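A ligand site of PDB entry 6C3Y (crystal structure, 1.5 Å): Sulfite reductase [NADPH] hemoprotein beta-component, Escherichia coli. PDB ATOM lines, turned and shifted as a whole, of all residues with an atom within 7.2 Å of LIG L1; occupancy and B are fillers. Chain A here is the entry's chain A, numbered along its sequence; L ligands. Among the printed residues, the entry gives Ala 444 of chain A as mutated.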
ATOM      1  N   ALA A 433      -6.069  -9.877 -32.101  1.00  0.00           N
ATOM      2  CA  ALA A 433      -6.530  -8.581 -31.574  1.00  0.00           C
ATOM      3  C   ALA A 433      -5.461  -7.966 -30.688  1.00  0.00           C
ATOM      4  O   ALA A 433      -4.631  -8.666 -30.110  1.00  0.00           O
ATOM      5  CB  ALA A 433      -7.821  -8.761 -30.803  1.00  0.00           C
ATOM      6  N   CYS A 434      -5.499  -6.640 -30.538  1.00  0.00           N
ATOM      7  CA  CYS A 434      -4.618  -5.969 -29.574  1.00  0.00           C
ATOM      8  C   CYS A 434      -5.210  -6.027 -28.163  1.00  0.00           C
ATOM      9  O   CYS A 434      -6.333  -6.507 -27.952  1.00  0.00           O
ATOM     10  CB  CYS A 434      -4.408  -4.505 -29.977  1.00  0.00           C
ATOM     11  SG  CYS A 434      -5.910  -3.505 -29.669  1.00  0.00           S
ATOM     12  N   VAL A 435      -4.456  -5.490 -27.191  1.00  0.00           N
ATOM     13  CA  VAL A 435      -4.866  -5.517 -25.785  1.00  0.00           C
ATOM     14  C   VAL A 435      -6.115  -4.685 -25.547  1.00  0.00           C
ATOM     15  O   VAL A 435      -7.096  -5.171 -24.970  1.00  0.00           O
ATOM     16  CB  VAL A 435      -3.711  -5.065 -24.886  1.00  0.00           C
ATOM     17  CG1 VAL A 435      -4.176  -4.924 -23.443  1.00  0.00           C
ATOM     18  CG2 VAL A 435      -2.531  -6.080 -24.975  1.00  0.00           C
ATOM     19  N   SER A 436      -6.072  -3.410 -25.928  1.00  0.00           N
ATOM     20  CA  SER A 436      -7.210  -2.482 -25.739  1.00  0.00           C
ATOM     21  C   SER A 436      -7.664  -2.451 -24.261  1.00  0.00           C
ATOM     22  O   SER A 436      -6.848  -2.574 -23.339  1.00  0.00           O
ATOM     23  CB  SER A 436      -8.298  -2.862 -26.732  1.00  0.00           C
ATOM     24  OG  SER A 436      -9.411  -1.950 -26.661  1.00  0.00           O
ATOM     25  N   PHE A 437      -8.961  -2.286 -24.019  1.00  0.00           N
ATOM     26  CA  PHE A 437      -9.493  -2.301 -22.661  1.00  0.00           C
ATOM     27  C   PHE A 437      -9.231  -3.662 -22.012  1.00  0.00           C
ATOM     28  O   PHE A 437      -9.310  -4.680 -22.687  1.00  0.00           O
ATOM     29  CB  PHE A 437     -10.996  -2.039 -22.671  1.00  0.00           C
ATOM     30  CG  PHE A 437     -11.400  -0.711 -23.257  1.00  0.00           C
ATOM     31  CD1 PHE A 437     -11.107   0.472 -22.614  1.00  0.00           C
ATOM     32  CD2 PHE A 437     -12.093  -0.667 -24.458  1.00  0.00           C
ATOM     33  CE1 PHE A 437     -11.495   1.704 -23.168  1.00  0.00           C
ATOM     34  CE2 PHE A 437     -12.471   0.539 -25.021  1.00  0.00           C
ATOM     35  CZ  PHE A 437     -12.183   1.725 -24.362  1.00  0.00           C
ATOM     36  N   THR A 439      -6.799  -2.196 -19.967  1.00  0.00           N
ATOM     37  CA  THR A 439      -5.565  -1.551 -19.556  1.00  0.00           C
ATOM     38  C   THR A 439      -5.055  -0.475 -20.508  1.00  0.00           C
ATOM     39  O   THR A 439      -4.307   0.406 -20.065  1.00  0.00           O
ATOM     40  CB  THR A 439      -4.448  -2.576 -19.366  1.00  0.00           C
ATOM     41  OG1 THR A 439      -4.344  -3.368 -20.566  1.00  0.00           O
ATOM     42  CG2 THR A 439      -4.733  -3.511 -18.171  1.00  0.00           C
ATOM     43  N   CYS A 440      -5.407  -0.514 -21.788  1.00  0.00           N
ATOM     44  CA  CYS A 440      -4.852   0.487 -22.704  1.00  0.00           C
ATOM     45  C   CYS A 440      -5.484   1.856 -22.481  1.00  0.00           C
ATOM     46  O   CYS A 440      -6.707   1.982 -22.591  1.00  0.00           O
ATOM     47  CB  CYS A 440      -5.039   0.089 -24.163  1.00  0.00           C
ATOM     48  SG  CYS A 440      -4.162   1.237 -25.190  1.00  0.00           S
ATOM     49  N   PRO A 441      -4.705   2.909 -22.233  1.00  0.00           N
ATOM     50  CA  PRO A 441      -5.304   4.248 -22.049  1.00  0.00           C
ATOM     51  C   PRO A 441      -5.784   4.910 -23.339  1.00  0.00           C
ATOM     52  O   PRO A 441      -6.455   5.943 -23.269  1.00  0.00           O
ATOM     53  CB  PRO A 441      -4.172   5.042 -21.406  1.00  0.00           C
ATOM     54  CG  PRO A 441      -2.930   4.402 -21.936  1.00  0.00           C
ATOM     55  CD  PRO A 441      -3.242   2.934 -22.052  1.00  0.00           C
ATOM     56  N   LEU A 442      -5.431   4.364 -24.505  1.00  0.00           N
ATOM     57  CA  LEU A 442      -5.762   4.939 -25.797  1.00  0.00           C
ATOM     58  C   LEU A 442      -6.941   4.233 -26.487  1.00  0.00           C
ATOM     59  O   LEU A 442      -7.350   4.675 -27.558  1.00  0.00           O
ATOM     60  CB  LEU A 442      -4.524   4.885 -26.706  1.00  0.00           C
ATOM     61  CG  LEU A 442      -3.271   5.448 -26.042  1.00  0.00           C
ATOM     62  CD1 LEU A 442      -2.074   5.396 -26.970  1.00  0.00           C
ATOM     63  CD2 LEU A 442      -3.499   6.889 -25.500  1.00  0.00           C
ATOM     64  N   ALA A 443      -7.476   3.174 -25.898  1.00  0.00           N
ATOM     65  CA  ALA A 443      -8.476   2.354 -26.575  1.00  0.00           C
ATOM     66  C   ALA A 443      -9.731   3.144 -26.928  1.00  0.00           C
ATOM     67  O   ALA A 443     -10.247   3.917 -26.110  1.00  0.00           O
ATOM     68  CB  ALA A 443      -8.856   1.165 -25.699  1.00  0.00           C
ATOM     69  N   ALA A 444     -10.245   2.909 -28.128  1.00  0.00           N
ATOM     70  CA  ALA A 444     -11.560   3.392 -28.518  1.00  0.00           C
ATOM     71  C   ALA A 444     -12.634   2.310 -28.443  1.00  0.00           C
ATOM     72  O   ALA A 444     -13.753   2.600 -28.001  1.00  0.00           O
ATOM     73  CB  ALA A 444     -11.523   3.997 -29.926  1.00  0.00           C
ATOM     74  N   ALA A 445     -12.318   1.076 -28.862  1.00  0.00           N
ATOM     75  CA  ALA A 445     -13.243  -0.051 -28.811  1.00  0.00           C
ATOM     76  C   ALA A 445     -12.501  -1.258 -28.276  1.00  0.00           C
ATOM     77  O   ALA A 445     -11.285  -1.368 -28.444  1.00  0.00           O
ATOM     78  CB  ALA A 445     -13.814  -0.427 -30.189  1.00  0.00           C
ATOM     79  N   ALA A 447     -10.929  -4.913 -28.090  1.00  0.00           N
ATOM     80  CA  ALA A 447     -10.312  -5.756 -29.108  1.00  0.00           C
ATOM     81  C   ALA A 447     -10.090  -7.154 -28.532  1.00  0.00           C
ATOM     82  O   ALA A 447     -10.866  -8.046 -28.845  1.00  0.00           O
ATOM     83  CB  ALA A 447      -9.012  -5.135 -29.611  1.00  0.00           C
ATOM     84  N   VAL A 476      -8.511  -7.396 -35.242  1.00  0.00           N
ATOM     85  CA  VAL A 476      -9.216  -6.289 -34.588  1.00  0.00           C
ATOM     86  C   VAL A 476      -8.202  -5.442 -33.845  1.00  0.00           C
ATOM     87  O   VAL A 476      -7.449  -5.945 -33.012  1.00  0.00           O
ATOM     88  CB  VAL A 476     -10.307  -6.804 -33.637  1.00  0.00           C
ATOM     89  CG1 VAL A 476     -11.105  -5.643 -33.048  1.00  0.00           C
ATOM     90  CG2 VAL A 476     -11.234  -7.770 -34.364  1.00  0.00           C
ATOM     91  N   THR A 477      -8.200  -4.145 -34.108  1.00  0.00           N
ATOM     92  CA  THR A 477      -7.318  -3.233 -33.377  1.00  0.00           C
ATOM     93  C   THR A 477      -8.204  -2.173 -32.731  1.00  0.00           C
ATOM     94  O   THR A 477      -9.170  -1.707 -33.349  1.00  0.00           O
ATOM     95  CB  THR A 477      -6.225  -2.669 -34.338  1.00  0.00           C
ATOM     96  OG1 THR A 477      -5.077  -2.202 -33.617  1.00  0.00           O
ATOM     97  CG2 THR A 477      -6.753  -1.556 -35.292  1.00  0.00           C
ATOM     98  N   GLY A 478      -7.913  -1.859 -31.463  1.00  0.00           N
ATOM     99  CA  GLY A 478      -8.840  -1.096 -30.634  1.00  0.00           C
ATOM    100  C   GLY A 478      -8.871   0.385 -30.911  1.00  0.00           C
ATOM    101  O   GLY A 478      -9.769   1.101 -30.427  1.00  0.00           O
ATOM    102  N   CYS A 479      -7.914   0.873 -31.681  1.00  0.00           N
ATOM    103  CA  CYS A 479      -7.841   2.254 -32.101  1.00  0.00           C
ATOM    104  C   CYS A 479      -6.878   2.307 -33.274  1.00  0.00           C
ATOM    105  O   CYS A 479      -6.240   1.285 -33.603  1.00  0.00           O
ATOM    106  CB  CYS A 479      -7.384   3.167 -30.927  1.00  0.00           C
ATOM    107  SG  CYS A 479      -5.580   3.319 -30.688  1.00  0.00           S
ATOM    108  N   PRO A 480      -6.761   3.439 -33.964  1.00  0.00           N
ATOM    109  CA  PRO A 480      -6.036   3.434 -35.240  1.00  0.00           C
ATOM    110  C   PRO A 480      -4.519   3.437 -35.100  1.00  0.00           C
ATOM    111  O   PRO A 480      -3.820   3.341 -36.116  1.00  0.00           O
ATOM    112  CB  PRO A 480      -6.553   4.697 -35.934  1.00  0.00           C
ATOM    113  CG  PRO A 480      -6.902   5.599 -34.809  1.00  0.00           C
ATOM    114  CD  PRO A 480      -7.480   4.711 -33.759  1.00  0.00           C
ATOM    115  N   ASN A 481      -3.976   3.474 -33.884  1.00  0.00           N
ATOM    116  CA  ASN A 481      -2.549   3.199 -33.696  1.00  0.00           C
ATOM    117  C   ASN A 481      -2.165   1.884 -34.354  1.00  0.00           C
ATOM    118  O   ASN A 481      -1.058   1.770 -34.888  1.00  0.00           O
ATOM    119  CB  ASN A 481      -2.215   3.173 -32.222  1.00  0.00           C
ATOM    120  CG  ASN A 481      -2.172   4.581 -31.632  1.00  0.00           C
ATOM    121  OD1 ASN A 481      -1.926   5.570 -32.350  1.00  0.00           O
ATOM    122  ND2 ASN A 481      -2.384   4.683 -30.336  1.00  0.00           N
ATOM    123  N   GLY A 482      -3.052   0.892 -34.322  1.00  0.00           N
ATOM    124  CA  GLY A 482      -2.911  -0.240 -35.225  1.00  0.00           C
ATOM    125  C   GLY A 482      -2.148  -1.416 -34.691  1.00  0.00           C
ATOM    126  O   GLY A 482      -1.715  -2.252 -35.489  1.00  0.00           O
ATOM    127  N   CYS A 483      -1.984  -1.512 -33.371  1.00  0.00           N
ATOM    128  CA  CYS A 483      -1.165  -2.550 -32.745  1.00  0.00           C
ATOM    129  C   CYS A 483      -1.632  -3.950 -33.103  1.00  0.00           C
ATOM    130  O   CYS A 483      -0.815  -4.870 -33.134  1.00  0.00           O
ATOM    131  CB  CYS A 483      -1.162  -2.449 -31.234  1.00  0.00           C
ATOM    132  SG  CYS A 483      -0.876  -0.752 -30.639  1.00  0.00           S
ATOM    133  N   GLY A 484      -2.940  -4.148 -33.321  1.00  0.00           N
ATOM    134  CA  GLY A 484      -3.435  -5.456 -33.715  1.00  0.00           C
ATOM    135  C   GLY A 484      -3.102  -5.833 -35.153  1.00  0.00           C
ATOM    136  O   GLY A 484      -3.398  -6.962 -35.568  1.00  0.00           O
ATOM    137  N   ARG A 485      -2.497  -4.913 -35.912  1.00  0.00           N
ATOM    138  CA  ARG A 485      -2.104  -5.118 -37.320  1.00  0.00           C
ATOM    139  C   ARG A 485      -3.298  -5.426 -38.220  1.00  0.00           C
ATOM    140  O   ARG A 485      -3.205  -6.172 -39.212  1.00  0.00           O
ATOM    141  CB  ARG A 485      -0.983  -6.174 -37.456  1.00  0.00           C
ATOM    142  CG  ARG A 485       0.287  -5.763 -36.629  1.00  0.00           C
ATOM    143  CD  ARG A 485       1.579  -6.440 -37.160  1.00  0.00           C
ATOM    144  NE  ARG A 485       1.563  -7.898 -37.033  1.00  0.00           N
ATOM    145  CZ  ARG A 485       2.154  -8.591 -36.072  1.00  0.00           C
ATOM    146  NH1 ARG A 485       2.813  -7.987 -35.076  1.00  0.00           N
ATOM    147  NH2 ARG A 485       2.107  -9.923 -36.112  1.00  0.00           N
HETATM  148 FE1  LIG L   1      -5.081  -1.366 -29.227  1.00  0.00          FE
HETATM  149 FE2  LIG L   1      -4.257   0.330 -27.316  1.00  0.00          FE
HETATM  150 FE3  LIG L   1      -4.968   1.301 -29.741  1.00  0.00          FE
HETATM  151 FE4  LIG L   1      -2.741  -0.215 -29.470  1.00  0.00          FE
HETATM  152  S1  LIG L   1      -3.085   1.737 -28.614  1.00  0.00           S
HETATM  153  S2  LIG L   1      -4.324  -0.351 -31.041  1.00  0.00           S
HETATM  154  S3  LIG L   1      -3.379  -1.620 -27.829  1.00  0.00           S
HETATM  155  S4  LIG L   1      -6.265   0.218 -28.283  1.00  0.00           S
HETATM  156 FE1  LG2 L   2       1.636  -0.791 -29.700  1.00  0.00          FE
HETATM  157  C1  LG2 L   2       1.123   2.151 -28.115  1.00  0.00           C
HETATM  158  C2  LG2 L   2       0.215  -2.465 -27.067  1.00  0.00           C
HETATM  159  C3  LG2 L   2       2.305  -3.794 -31.192  1.00  0.00           C
HETATM  160  C4  LG2 L   2       1.724   0.788 -32.711  1.00  0.00           C
HETATM  161  N1  LG2 L   2       0.875  -0.268 -27.908  1.00  0.00           N
HETATM  162  C5  LG2 L   2       0.815   1.002 -27.399  1.00  0.00           C
HETATM  163  C6  LG2 L   2       0.484   1.023 -25.912  1.00  0.00           C
HETATM  164  C7  LG2 L   2       1.777   1.107 -25.099  1.00  0.00           C
HETATM  165  C8  LG2 L   2      -0.470   2.184 -25.532  1.00  0.00           C
HETATM  166  C9  LG2 L   2       0.199   3.425 -24.946  1.00  0.00           C
HETATM  167  O1  LG2 L   2       0.945   4.169 -25.622  1.00  0.00           O
HETATM  168  O2  LG2 L   2      -0.025   3.767 -23.763  1.00  0.00           O
HETATM  169  C10 LG2 L   2      -0.210  -0.308 -25.794  1.00  0.00           C
HETATM  170  C11 LG2 L   2      -0.396  -0.843 -24.398  1.00  0.00           C
HETATM  171  C12 LG2 L   2      -1.653  -1.718 -24.314  1.00  0.00           C
HETATM  172  C13 LG2 L   2      -1.691  -2.413 -22.973  1.00  0.00           C
HETATM  173  O3  LG2 L   2      -2.476  -2.064 -22.064  1.00  0.00           O
HETATM  174  O4  LG2 L   2      -0.927  -3.369 -22.772  1.00  0.00           O
HETATM  175  C14 LG2 L   2       0.275  -1.086 -26.985  1.00  0.00           C
HETATM  176  N2  LG2 L   2       1.388  -2.712 -29.201  1.00  0.00           N
HETATM  177  C15 LG2 L   2       0.780  -3.236 -28.093  1.00  0.00           C
HETATM  178  C16 LG2 L   2       0.801  -4.754 -28.107  1.00  0.00           C
HETATM  179  C17 LG2 L   2       0.931  -5.360 -26.697  1.00  0.00           C
HETATM  180  C18 LG2 L   2      -0.470  -5.298 -28.781  1.00  0.00           C
HETATM  181  C19 LG2 L   2      -0.726  -6.775 -28.618  1.00  0.00           C
HETATM  182  O5  LG2 L   2      -1.869  -7.157 -28.325  1.00  0.00           O
HETATM  183  O6  LG2 L   2       0.157  -7.629 -28.792  1.00  0.00           O
HETATM  184  C20 LG2 L   2       2.030  -4.951 -28.944  1.00  0.00           C
HETATM  185  C21 LG2 L   2       3.304  -4.979 -28.124  1.00  0.00           C
HETATM  186  C22 LG2 L   2       4.485  -5.236 -29.067  1.00  0.00           C
HETATM  187  C23 LG2 L   2       5.765  -5.115 -28.278  1.00  0.00           C
HETATM  188  O7  LG2 L   2       6.129  -6.065 -27.553  1.00  0.00           O
HETATM  189  O8  LG2 L   2       6.488  -4.088 -28.338  1.00  0.00           O
HETATM  190  C24 LG2 L   2       1.927  -3.773 -29.856  1.00  0.00           C
HETATM  191  N3  LG2 L   2       1.975  -1.385 -31.576  1.00  0.00           N
HETATM  192  C25 LG2 L   2       2.198  -2.653 -32.004  1.00  0.00           C
HETATM  193  C26 LG2 L   2       2.329  -2.704 -33.472  1.00  0.00           C
HETATM  194  C27 LG2 L   2       2.403  -3.947 -34.297  1.00  0.00           C
HETATM  195  C28 LG2 L   2       3.846  -4.383 -34.440  1.00  0.00           C
HETATM  196  O9  LG2 L   2       4.809  -3.675 -34.064  1.00  0.00           O
HETATM  197  O10 LG2 L   2       4.067  -5.483 -34.992  1.00  0.00           O
HETATM  198  C29 LG2 L   2       2.044  -1.382 -33.971  1.00  0.00           C
HETATM  199  C30 LG2 L   2       1.737  -1.002 -35.392  1.00  0.00           C
HETATM  200  C31 LG2 L   2       3.000  -1.052 -36.281  1.00  0.00           C
HETATM  201  C32 LG2 L   2       3.584   0.334 -36.267  1.00  0.00           C
HETATM  202  O11 LG2 L   2       4.228   0.736 -35.261  1.00  0.00           O
HETATM  203  O12 LG2 L   2       3.378   1.121 -37.216  1.00  0.00           O
HETATM  204  C33 LG2 L   2       1.903  -0.593 -32.707  1.00  0.00           C
HETATM  205  N4  LG2 L   2       1.609   1.115 -30.274  1.00  0.00           N
HETATM  206  C34 LG2 L   2       1.596   1.579 -31.567  1.00  0.00           C
HETATM  207  C35 LG2 L   2       1.432   3.059 -31.638  1.00  0.00           C
HETATM  208  C36 LG2 L   2       1.342   3.980 -32.834  1.00  0.00           C
HETATM  209  C37 LG2 L   2       2.770   4.244 -33.304  1.00  0.00           C
HETATM  210  C38 LG2 L   2       2.857   5.286 -34.386  1.00  0.00           C
HETATM  211  O13 LG2 L   2       3.774   5.219 -35.236  1.00  0.00           O
HETATM  212  O14 LG2 L   2       2.040   6.227 -34.476  1.00  0.00           O
HETATM  213  C39 LG2 L   2       1.248   3.433 -30.246  1.00  0.00           C
HETATM  214  C40 LG2 L   2       0.937   4.818 -29.735  1.00  0.00           C
HETATM  215  C41 LG2 L   2       2.210   5.643 -29.661  1.00  0.00           C
HETATM  216  O15 LG2 L   2       3.358   5.181 -29.840  1.00  0.00           O
HETATM  217  O16 LG2 L   2       2.128   6.856 -29.400  1.00  0.00           O
HETATM  218  C42 LG2 L   2       1.354   2.183 -29.478  1.00  0.00           C
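Leu 442 touches LIG L1 (CB to S1, 3.95 Å). CA of Ala 443 touches S4 of LIG L1, at 3.5 Å. Gly 478 touches LIG L1 (N to FE1, 3.6 Å). Hydrophobic or aromatic side chains that line LIG L1: Leu 442 and Ala 443. The nearest printed residue that does not touch LIG L1 is Val 435 (4.1 Å).
The backbone NH (N) of Cys 483 sits close to a sulfur (S2) of LIG L1, at 3.5 Å. An iron atom (FE4) of LIG L1 is bound by the side-chain sulfur (SG) of Cys 483 (2.3 Å). The side-chain sulfur (SG) of Cys 479 is bound to an iron atom (FE3) of LIG L1 (2.3 Å). SG of Cys 440 binds FE2 of LIG L1 (2.3 Å). The side-chain sulfur (SG) of Cys 434 is bound to an iron atom (FE1) of LIG L1, 2.3 Å away. OG1 of Thr 477 sits close to S2 of LIG L1 (3.3 Å). The side-chain amide nitrogen (ND2) of Asn 481 lies close to a sulfur (S1) of LIG L1 (3.5 Å). A sulfur (S2) of LIG L1 lies close to the backbone NH of Gly 482, at 3.7 Å. The backbone NH (N) of Ser 436 sits close to a sulfur (S3) of LIG L1 (3.8 Å). The side-chain sulfur of Cys 483 is bound to an iron atom (FE1) of LG2 L2 (2.7 Å). The backbone NH of Cys 440 sits at hydrogen-bond distance from an oxygen (O3) of LG2 L2. O5 of LG2 L2 is in hydrogen-bond range of N of Val 435, 3.3 Å away. OG1 of Thr 439 sits at hydrogen-bond distance from O3 of LG2 L2 (2.7 Å). The guanidinium group of Arg 485 is in salt-bridge range of an oxygen (O10) of LG2 L2, at 2.8 Å.
OG1 of Thr 477 sits at hydrogen-bond distance from N of Cys 483 (3.2 Å). The side-chain sulfur (SG) of Cys 479 lies close to the side-chain amide nitrogen (ND2) of Asn 481 (3.5 Å). N of Leu 442 sits close to SG of Cys 440 (3.4 Å). The side-chain sulfur (SG) of Cys 434 lies close to the backbone NH (N) of Gly 478. SG of Cys 434 lies close to N of Ser 436 (3.7 Å). The side-chain hydroxyl of Thr 477 lies within hydrogen-bond range of the backbone NH of Gly 484 (2.9 Å). The backbone NH (N) of Ala 444 sits at hydrogen-bond distance from the backbone carbonyl oxygen (O) of Gly 478. O of Gly 478 is in hydrogen-bond range of N of Ala 445 (3.0 Å).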
